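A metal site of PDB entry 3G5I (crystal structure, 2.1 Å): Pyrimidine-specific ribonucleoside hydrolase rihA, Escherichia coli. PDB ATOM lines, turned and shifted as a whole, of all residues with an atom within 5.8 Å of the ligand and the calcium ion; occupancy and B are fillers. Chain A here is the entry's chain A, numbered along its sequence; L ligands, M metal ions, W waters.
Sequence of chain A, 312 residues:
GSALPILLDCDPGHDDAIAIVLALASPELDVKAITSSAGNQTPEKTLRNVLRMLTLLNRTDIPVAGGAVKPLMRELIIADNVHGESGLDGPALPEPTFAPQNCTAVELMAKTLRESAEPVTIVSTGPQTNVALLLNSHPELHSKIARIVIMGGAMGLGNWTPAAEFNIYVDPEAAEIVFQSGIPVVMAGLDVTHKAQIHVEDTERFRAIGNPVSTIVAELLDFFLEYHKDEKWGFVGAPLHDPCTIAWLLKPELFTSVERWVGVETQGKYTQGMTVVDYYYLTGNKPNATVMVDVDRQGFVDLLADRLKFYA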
ATOM      1  N   CYS A  10      13.035  -2.708  18.451  1.00  0.00           N
ATOM      2  CA  CYS A  10      14.030  -1.760  17.916  1.00  0.00           C
ATOM      3  C   CYS A  10      15.477  -2.154  18.242  1.00  0.00           C
ATOM      4  O   CYS A  10      15.713  -3.026  19.053  1.00  0.00           O
ATOM      5  CB  CYS A  10      13.701  -0.337  18.405  1.00  0.00           C
ATOM      6  SG  CYS A  10      13.898  -0.087  20.145  1.00  0.00           S
ATOM      7  N   ASP A  11      16.422  -1.548  17.558  1.00  0.00           N
ATOM      8  CA  ASP A  11      17.782  -1.925  17.717  1.00  0.00           C
ATOM      9  C   ASP A  11      18.716  -0.734  17.907  1.00  0.00           C
ATOM     10  O   ASP A  11      19.621  -0.537  17.111  1.00  0.00           O
ATOM     11  CB  ASP A  11      18.210  -2.813  16.524  1.00  0.00           C
ATOM     12  CG  ASP A  11      18.209  -2.042  15.192  1.00  0.00           C
ATOM     13  OD1 ASP A  11      17.340  -1.141  15.043  1.00  0.00           O
ATOM     14  OD2 ASP A  11      19.062  -2.326  14.292  1.00  0.00           O
ATOM     15  N   PRO A  12      18.553   0.036  19.011  1.00  0.00           N
ATOM     16  CA  PRO A  12      19.228   1.306  19.166  1.00  0.00           C
ATOM     17  C   PRO A  12      20.744   1.188  19.204  1.00  0.00           C
ATOM     18  O   PRO A  12      21.242   0.318  19.902  1.00  0.00           O
ATOM     19  CB  PRO A  12      18.683   1.841  20.514  1.00  0.00           C
ATOM     20  CG  PRO A  12      17.521   1.037  20.864  1.00  0.00           C
ATOM     21  CD  PRO A  12      17.760  -0.298  20.216  1.00  0.00           C
ATOM     22  N   GLY A  13      21.481   1.999  18.426  1.00  0.00           N
ATOM     23  CA  GLY A  13      20.980   2.839  17.304  1.00  0.00           C
ATOM     24  C   GLY A  13      20.380   4.227  17.597  1.00  0.00           C
ATOM     25  O   GLY A  13      19.336   4.374  18.245  1.00  0.00           O
ATOM     26  N   ASP A  15      18.805   6.573  15.856  1.00  0.00           N
ATOM     27  CA  ASP A  15      17.472   6.949  15.453  1.00  0.00           C
ATOM     28  C   ASP A  15      16.350   6.186  16.175  1.00  0.00           C
ATOM     29  O   ASP A  15      15.339   6.774  16.521  1.00  0.00           O
ATOM     30  CB  ASP A  15      17.337   7.005  13.908  1.00  0.00           C
ATOM     31  CG  ASP A  15      17.595   5.692  13.256  1.00  0.00           C
ATOM     32  OD1 ASP A  15      18.498   4.949  13.699  1.00  0.00           O
ATOM     33  OD2 ASP A  15      16.881   5.405  12.282  1.00  0.00           O
ATOM     34  N   ASP A  16      16.548   4.907  16.452  1.00  0.00           N
ATOM     35  CA  ASP A  16      15.672   4.174  17.350  1.00  0.00           C
ATOM     36  C   ASP A  16      15.528   4.901  18.673  1.00  0.00           C
ATOM     37  O   ASP A  16      14.406   5.056  19.168  1.00  0.00           O
ATOM     38  CB  ASP A  16      16.246   2.774  17.683  1.00  0.00           C
ATOM     39  CG  ASP A  16      16.554   1.955  16.428  1.00  0.00           C
ATOM     40  OD1 ASP A  16      17.683   2.090  15.856  1.00  0.00           O
ATOM     41  OD2 ASP A  16      15.658   1.182  16.032  1.00  0.00           O
ATOM     42  N   ASN A  40      21.618  -3.116  14.037  1.00  0.00           N
ATOM     43  CA  ASN A  40      22.537  -1.973  14.297  1.00  0.00           C
ATOM     44  C   ASN A  40      23.739  -2.409  15.153  1.00  0.00           C
ATOM     45  O   ASN A  40      24.871  -1.969  14.894  1.00  0.00           O
ATOM     46  CB  ASN A  40      21.826  -0.751  14.945  1.00  0.00           C
ATOM     47  CG  ASN A  40      21.171   0.203  13.907  1.00  0.00           C
ATOM     48  OD1 ASN A  40      21.572   0.235  12.722  1.00  0.00           O
ATOM     49  ND2 ASN A  40      20.118   0.942  14.331  1.00  0.00           N
ATOM     50  N   ALA A  79      25.229  -2.841  11.693  1.00  0.00           N
ATOM     51  CA  ALA A  79      25.573  -1.493  11.197  1.00  0.00           C
ATOM     52  C   ALA A  79      26.620  -0.872  12.152  1.00  0.00           C
ATOM     53  O   ALA A  79      26.328   0.041  12.957  1.00  0.00           O
ATOM     54  CB  ALA A  79      24.330  -0.631  11.038  1.00  0.00           C
ATOM     55  N   VAL A  82      28.905   2.951  11.288  1.00  0.00           N
ATOM     56  CA  VAL A  82      27.842   3.948  11.061  1.00  0.00           C
ATOM     57  C   VAL A  82      27.305   4.514  12.401  1.00  0.00           C
ATOM     58  O   VAL A  82      27.221   5.750  12.575  1.00  0.00           O
ATOM     59  CB  VAL A  82      26.637   3.342  10.253  1.00  0.00           C
ATOM     60  CG1 VAL A  82      25.465   4.305  10.212  1.00  0.00           C
ATOM     61  CG2 VAL A  82      27.071   2.928   8.855  1.00  0.00           C
ATOM     62  N   HIS A  83      26.968   3.602  13.316  1.00  0.00           N
ATOM     63  CA  HIS A  83      26.397   3.888  14.649  1.00  0.00           C
ATOM     64  C   HIS A  83      27.450   3.885  15.785  1.00  0.00           C
ATOM     65  O   HIS A  83      27.116   4.066  16.978  1.00  0.00           O
ATOM     66  CB  HIS A  83      25.276   2.884  14.952  1.00  0.00           C
ATOM     67  CG  HIS A  83      24.106   3.007  14.038  1.00  0.00           C
ATOM     68  ND1 HIS A  83      23.083   3.918  14.249  1.00  0.00           N
ATOM     69  CD2 HIS A  83      23.806   2.374  12.871  1.00  0.00           C
ATOM     70  CE1 HIS A  83      22.198   3.827  13.266  1.00  0.00           C
ATOM     71  NE2 HIS A  83      22.613   2.900  12.418  1.00  0.00           N
ATOM     72  N   THR A 125      11.559  -1.224  14.246  1.00  0.00           N
ATOM     73  CA  THR A 125      12.484  -0.303  13.614  1.00  0.00           C
ATOM     74  C   THR A 125      13.897  -0.877  13.466  1.00  0.00           C
ATOM     75  O   THR A 125      14.836  -0.169  13.096  1.00  0.00           O
ATOM     76  CB  THR A 125      12.496   1.089  14.377  1.00  0.00           C
ATOM     77  OG1 THR A 125      12.979   0.951  15.724  1.00  0.00           O
ATOM     78  CG2 THR A 125      11.138   1.642  14.406  1.00  0.00           C
ATOM     79  N   GLY A 126      14.025  -2.165  13.763  1.00  0.00           N
ATOM     80  CA  GLY A 126      15.174  -2.899  13.339  1.00  0.00           C
ATOM     81  C   GLY A 126      14.785  -3.989  12.360  1.00  0.00           C
ATOM     82  O   GLY A 126      13.666  -4.004  11.845  1.00  0.00           O
ATOM     83  N   MET A 151      10.222   0.589  10.093  1.00  0.00           N
ATOM     84  CA  MET A 151      11.198   1.337   9.334  1.00  0.00           C
ATOM     85  C   MET A 151      12.029   0.269   8.597  1.00  0.00           C
ATOM     86  O   MET A 151      12.622  -0.664   9.202  1.00  0.00           O
ATOM     87  CB  MET A 151      12.057   2.239  10.221  1.00  0.00           C
ATOM     88  CG  MET A 151      12.931   3.198   9.371  1.00  0.00           C
ATOM     89  SD  MET A 151      14.284   2.289   8.586  1.00  0.00           S
ATOM     90  CE  MET A 151      14.326   3.130   6.992  1.00  0.00           C
ATOM     91  N   ASN A 159      20.348   1.338   0.703  1.00  0.00           N
ATOM     92  CA  ASN A 159      21.497   1.954   1.355  1.00  0.00           C
ATOM     93  C   ASN A 159      22.526   0.950   1.845  1.00  0.00           C
ATOM     94  O   ASN A 159      23.575   1.340   2.372  1.00  0.00           O
ATOM     95  CB  ASN A 159      21.058   2.938   2.500  1.00  0.00           C
ATOM     96  CG  ASN A 159      20.359   2.222   3.690  1.00  0.00           C
ATOM     97  OD1 ASN A 159      20.075   1.009   3.646  1.00  0.00           O
ATOM     98  ND2 ASN A 159      20.099   2.997   4.793  1.00  0.00           N
ATOM     99  N   TRP A 160      22.248  -0.342   1.666  1.00  0.00           N
ATOM    100  CA  TRP A 160      23.171  -1.343   2.152  1.00  0.00           C
ATOM    101  C   TRP A 160      23.866  -2.136   1.006  1.00  0.00           C
ATOM    102  O   TRP A 160      25.123  -2.201   0.924  1.00  0.00           O
ATOM    103  CB  TRP A 160      22.473  -2.276   3.135  1.00  0.00           C
ATOM    104  CG  TRP A 160      23.505  -3.058   3.917  1.00  0.00           C
ATOM    105  CD1 TRP A 160      23.778  -4.402   3.810  1.00  0.00           C
ATOM    106  CD2 TRP A 160      24.433  -2.525   4.887  1.00  0.00           C
ATOM    107  NE1 TRP A 160      24.833  -4.710   4.656  1.00  0.00           N
ATOM    108  CE2 TRP A 160      25.232  -3.588   5.332  1.00  0.00           C
ATOM    109  CE3 TRP A 160      24.673  -1.226   5.401  1.00  0.00           C
ATOM    110  CZ2 TRP A 160      26.287  -3.422   6.276  1.00  0.00           C
ATOM    111  CZ3 TRP A 160      25.688  -1.044   6.363  1.00  0.00           C
ATOM    112  CH2 TRP A 160      26.491  -2.139   6.778  1.00  0.00           C
ATOM    113  N   GLU A 165      17.748  -2.143   1.497  1.00  0.00           N
ATOM    114  CA  GLU A 165      17.945  -1.341   2.691  1.00  0.00           C
ATOM    115  C   GLU A 165      18.381  -2.262   3.824  1.00  0.00           C
ATOM    116  O   GLU A 165      18.044  -3.418   3.845  1.00  0.00           O
ATOM    117  CB  GLU A 165      16.670  -0.513   2.997  1.00  0.00           C
ATOM    118  CG  GLU A 165      16.682   0.348   4.296  1.00  0.00           C
ATOM    119  CD  GLU A 165      16.415  -0.469   5.559  1.00  0.00           C
ATOM    120  OE1 GLU A 165      15.657  -1.452   5.499  1.00  0.00           O
ATOM    121  OE2 GLU A 165      16.948  -0.112   6.620  1.00  0.00           O
ATOM    122  N   PHE A 166      19.160  -1.753   4.775  1.00  0.00           N
ATOM    123  CA  PHE A 166      19.803  -2.567   5.807  1.00  0.00           C
ATOM    124  C   PHE A 166      18.894  -3.482   6.644  1.00  0.00           C
ATOM    125  O   PHE A 166      19.129  -4.653   6.785  1.00  0.00           O
ATOM    126  CB  PHE A 166      20.574  -1.634   6.748  1.00  0.00           C
ATOM    127  CG  PHE A 166      21.198  -2.360   7.920  1.00  0.00           C
ATOM    128  CD1 PHE A 166      22.473  -2.932   7.800  1.00  0.00           C
ATOM    129  CD2 PHE A 166      20.530  -2.439   9.163  1.00  0.00           C
ATOM    130  CE1 PHE A 166      23.072  -3.619   8.868  1.00  0.00           C
ATOM    131  CE2 PHE A 166      21.115  -3.126  10.269  1.00  0.00           C
ATOM    132  CZ  PHE A 166      22.401  -3.708  10.121  1.00  0.00           C
ATOM    133  N   ASN A 167      17.884  -2.914   7.287  1.00  0.00           N
ATOM    134  CA  ASN A 167      16.976  -3.674   8.164  1.00  0.00           C
ATOM    135  C   ASN A 167      16.395  -4.856   7.460  1.00  0.00           C
ATOM    136  O   ASN A 167      16.278  -5.940   8.029  1.00  0.00           O
ATOM    137  CB  ASN A 167      15.823  -2.825   8.638  1.00  0.00           C
ATOM    138  CG  ASN A 167      16.204  -1.891   9.723  1.00  0.00           C
ATOM    139  OD1 ASN A 167      17.375  -1.859  10.233  1.00  0.00           O
ATOM    140  ND2 ASN A 167      15.224  -1.083  10.118  1.00  0.00           N
ATOM    141  N   LEU A 190      13.235   4.088   2.683  1.00  0.00           N
ATOM    142  CA  LEU A 190      14.180   5.155   2.361  1.00  0.00           C
ATOM    143  C   LEU A 190      13.516   6.251   1.497  1.00  0.00           C
ATOM    144  O   LEU A 190      13.918   7.399   1.509  1.00  0.00           O
ATOM    145  CB  LEU A 190      15.393   4.574   1.661  1.00  0.00           C
ATOM    146  CG  LEU A 190      16.215   3.635   2.545  1.00  0.00           C
ATOM    147  CD1 LEU A 190      17.425   3.119   1.758  1.00  0.00           C
ATOM    148  CD2 LEU A 190      16.643   4.270   3.903  1.00  0.00           C
ATOM    149  N   PHE A 224      25.861  11.579  13.975  1.00  0.00           N
ATOM    150  CA  PHE A 224      25.467  11.282  12.591  1.00  0.00           C
ATOM    151  C   PHE A 224      25.926  12.295  11.547  1.00  0.00           C
ATOM    152  O   PHE A 224      25.398  12.269  10.420  1.00  0.00           O
ATOM    153  CB  PHE A 224      23.958  11.231  12.431  1.00  0.00           C
ATOM    154  CG  PHE A 224      23.308   9.976  12.897  1.00  0.00           C
ATOM    155  CD1 PHE A 224      23.773   8.732  12.483  1.00  0.00           C
ATOM    156  CD2 PHE A 224      22.167  10.048  13.714  1.00  0.00           C
ATOM    157  CE1 PHE A 224      23.132   7.566  12.908  1.00  0.00           C
ATOM    158  CE2 PHE A 224      21.508   8.911  14.144  1.00  0.00           C
ATOM    159  CZ  PHE A 224      21.982   7.649  13.744  1.00  0.00           C
ATOM    160  N   HIS A 241      15.582   8.196  10.342  1.00  0.00           N
ATOM    161  CA  HIS A 241      14.751   7.119   9.815  1.00  0.00           C
ATOM    162  C   HIS A 241      13.656   6.682  10.794  1.00  0.00           C
ATOM    163  O   HIS A 241      12.449   6.813  10.532  1.00  0.00           O
ATOM    164  CB  HIS A 241      15.618   5.886   9.410  1.00  0.00           C
ATOM    165  CG  HIS A 241      16.772   6.225   8.495  1.00  0.00           C
ATOM    166  ND1 HIS A 241      16.628   6.302   7.126  1.00  0.00           N
ATOM    167  CD2 HIS A 241      18.074   6.464   8.761  1.00  0.00           C
ATOM    168  CE1 HIS A 241      17.809   6.579   6.581  1.00  0.00           C
ATOM    169  NE2 HIS A 241      18.685   6.730   7.560  1.00  0.00           N
ATOM    170  N   ASP A 242      14.085   6.147  11.939  1.00  0.00           N
ATOM    171  CA  ASP A 242      13.127   5.440  12.810  1.00  0.00           C
ATOM    172  C   ASP A 242      11.963   6.303  13.374  1.00  0.00           C
ATOM    173  O   ASP A 242      10.782   5.849  13.405  1.00  0.00           O
ATOM    174  CB  ASP A 242      13.921   4.694  13.902  1.00  0.00           C
ATOM    175  CG  ASP A 242      14.788   3.580  13.304  1.00  0.00           C
ATOM    176  OD1 ASP A 242      14.587   3.283  12.080  1.00  0.00           O
ATOM    177  OD2 ASP A 242      15.633   2.967  14.011  1.00  0.00           O
HETATM  178  O1  LIG L   1      18.513   2.393  12.606  1.00  0.00           O
HETATM  179  C1  LIG L   1      18.683   2.698  11.202  1.00  0.00           C
HETATM  180  C2  LIG L   1      17.324   2.532  10.493  1.00  0.00           C
HETATM  181  O2  LIG L   1      16.341   1.804  11.260  1.00  0.00           O
HETATM  182  C3  LIG L   1      19.642   1.695  10.528  1.00  0.00           C
HETATM  183  N1  LIG L   1      18.744   0.919   9.657  1.00  0.00           N
HETATM  184  C4  LIG L   1      17.648   1.754   9.201  1.00  0.00           C
HETATM  185  C5  LIG L   1      18.029   2.706   8.037  1.00  0.00           C
HETATM  186  O3  LIG L   1      18.596   1.950   6.963  1.00  0.00           O
HETATM  187  C6  LIG L   1      20.748   2.222   9.658  1.00  0.00           C
HETATM  188  C7  LIG L   1      21.615   1.273   9.100  1.00  0.00           C
HETATM  189  C8  LIG L   1      22.683   1.593   8.262  1.00  0.00           C
HETATM  190  C9  LIG L   1      22.885   2.941   7.939  1.00  0.00           C
HETATM  191  C10 LIG L   1      22.043   3.932   8.462  1.00  0.00           C
HETATM  192  N2  LIG L   1      22.309   5.207   8.110  1.00  0.00           N
HETATM  193  C11 LIG L   1      20.959   3.569   9.306  1.00  0.00           C
HETATM  194 CA    CA M   1      16.863   0.871  13.805  1.00  0.00          CA
HETATM  195  O   HOH W   1      18.207  -0.528  12.413  1.00  0.00           O
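OD1 of Asn 167 sits at hydrogen-bond distance from N1 of the ligand (3.2 Å). O3 of the ligand sits at hydrogen-bond distance from ND2 of Asn 159 (2.8 Å). N1 of the ligand lies within salt-bridge range of OE2 of Glu 165, 3.7 Å away. The side-chain amide nitrogen (ND2) of Asn 40 lies close to an oxygen (O1) of the ligand, 2.8 Å away. The side-chain carboxylate (OD1) of Asp 15 sits close to an oxygen (O1) of the ligand, at 2.8 Å. The side-chain sulfur (SD) of Met 151 sits close to an oxygen (O2) of the ligand, 3.4 Å away.
The backbone carbonyl oxygen (O) of Met 151 lies within hydrogen-bond range of the side-chain amide nitrogen (ND2) of Asn 167, 2.8 Å away. N of Asn 167 sits at hydrogen-bond distance from OE2 of Glu 165 (3.0 Å). The backbone NH (N) of Asp 242 sits at hydrogen-bond distance from the side-chain carboxylate (OD2) of Asp 15 (2.9 Å). N of Ala 79 lies within hydrogen-bond range of O of Asn 40, at 3.3 Å. The backbone carbonyl oxygen (O) of Thr 125 lies close to the side-chain amide nitrogen (ND2) of Asn 167. OD2 of Asp 11 is in hydrogen-bond range of N of Asn 40, at 2.7 Å. The side-chain amide oxygen (OD1) of Asn 159 sits at hydrogen-bond distance from the backbone NH (N) of Phe 166 (3.1 Å). The side-chain amide oxygen (OD1) of Asn 40 lies within hydrogen-bond range of a ring nitrogen (NE2) of His 83 (2.9 Å).
Residues that only touch the ligand: Ala 79, Val 82, His 83, Phe 166 and His 241. Hydrophobic or aromatic side chains within 4 Å of the ligand: Ala 79, Val 82, Met 151, Phe 166 and His 241. 14 residues have an atom within 4 Å of the ligand: Asp 15, Asp 16, Asn 40, Ala 79, Val 82, His 83, Thr 125, Met 151, Asn 159, Glu 165, Phe 166, Asn 167, His 241 and Asp 242. The nearest printed residue that does not touch the ligand is Leu 190 (4.3 Å).
ND2 of Asn 40 touches the calcium ion, at 3.3 Å. Of the 22 residues printed, 5 come within 4 Å of the calcium ion.
The calcium ion is bound by the backbone carbonyl oxygen (O) of Thr 125, water W1, the side-chain carboxylate (OD1) of Asp 11, the side-chain carboxylate (OD2) of Asp 242, the side-chain carboxylate (OD1) of Asp 16, an oxygen (O1) of the ligand, the side-chain carboxylate (OD2) of Asp 16 and an oxygen (O2) of the ligand.
Water W1 lies within hydrogen-bond range of OD1 of Asn 167, OD2 of Asp 11, ND2 of Asn 40 and N1 of the ligand.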
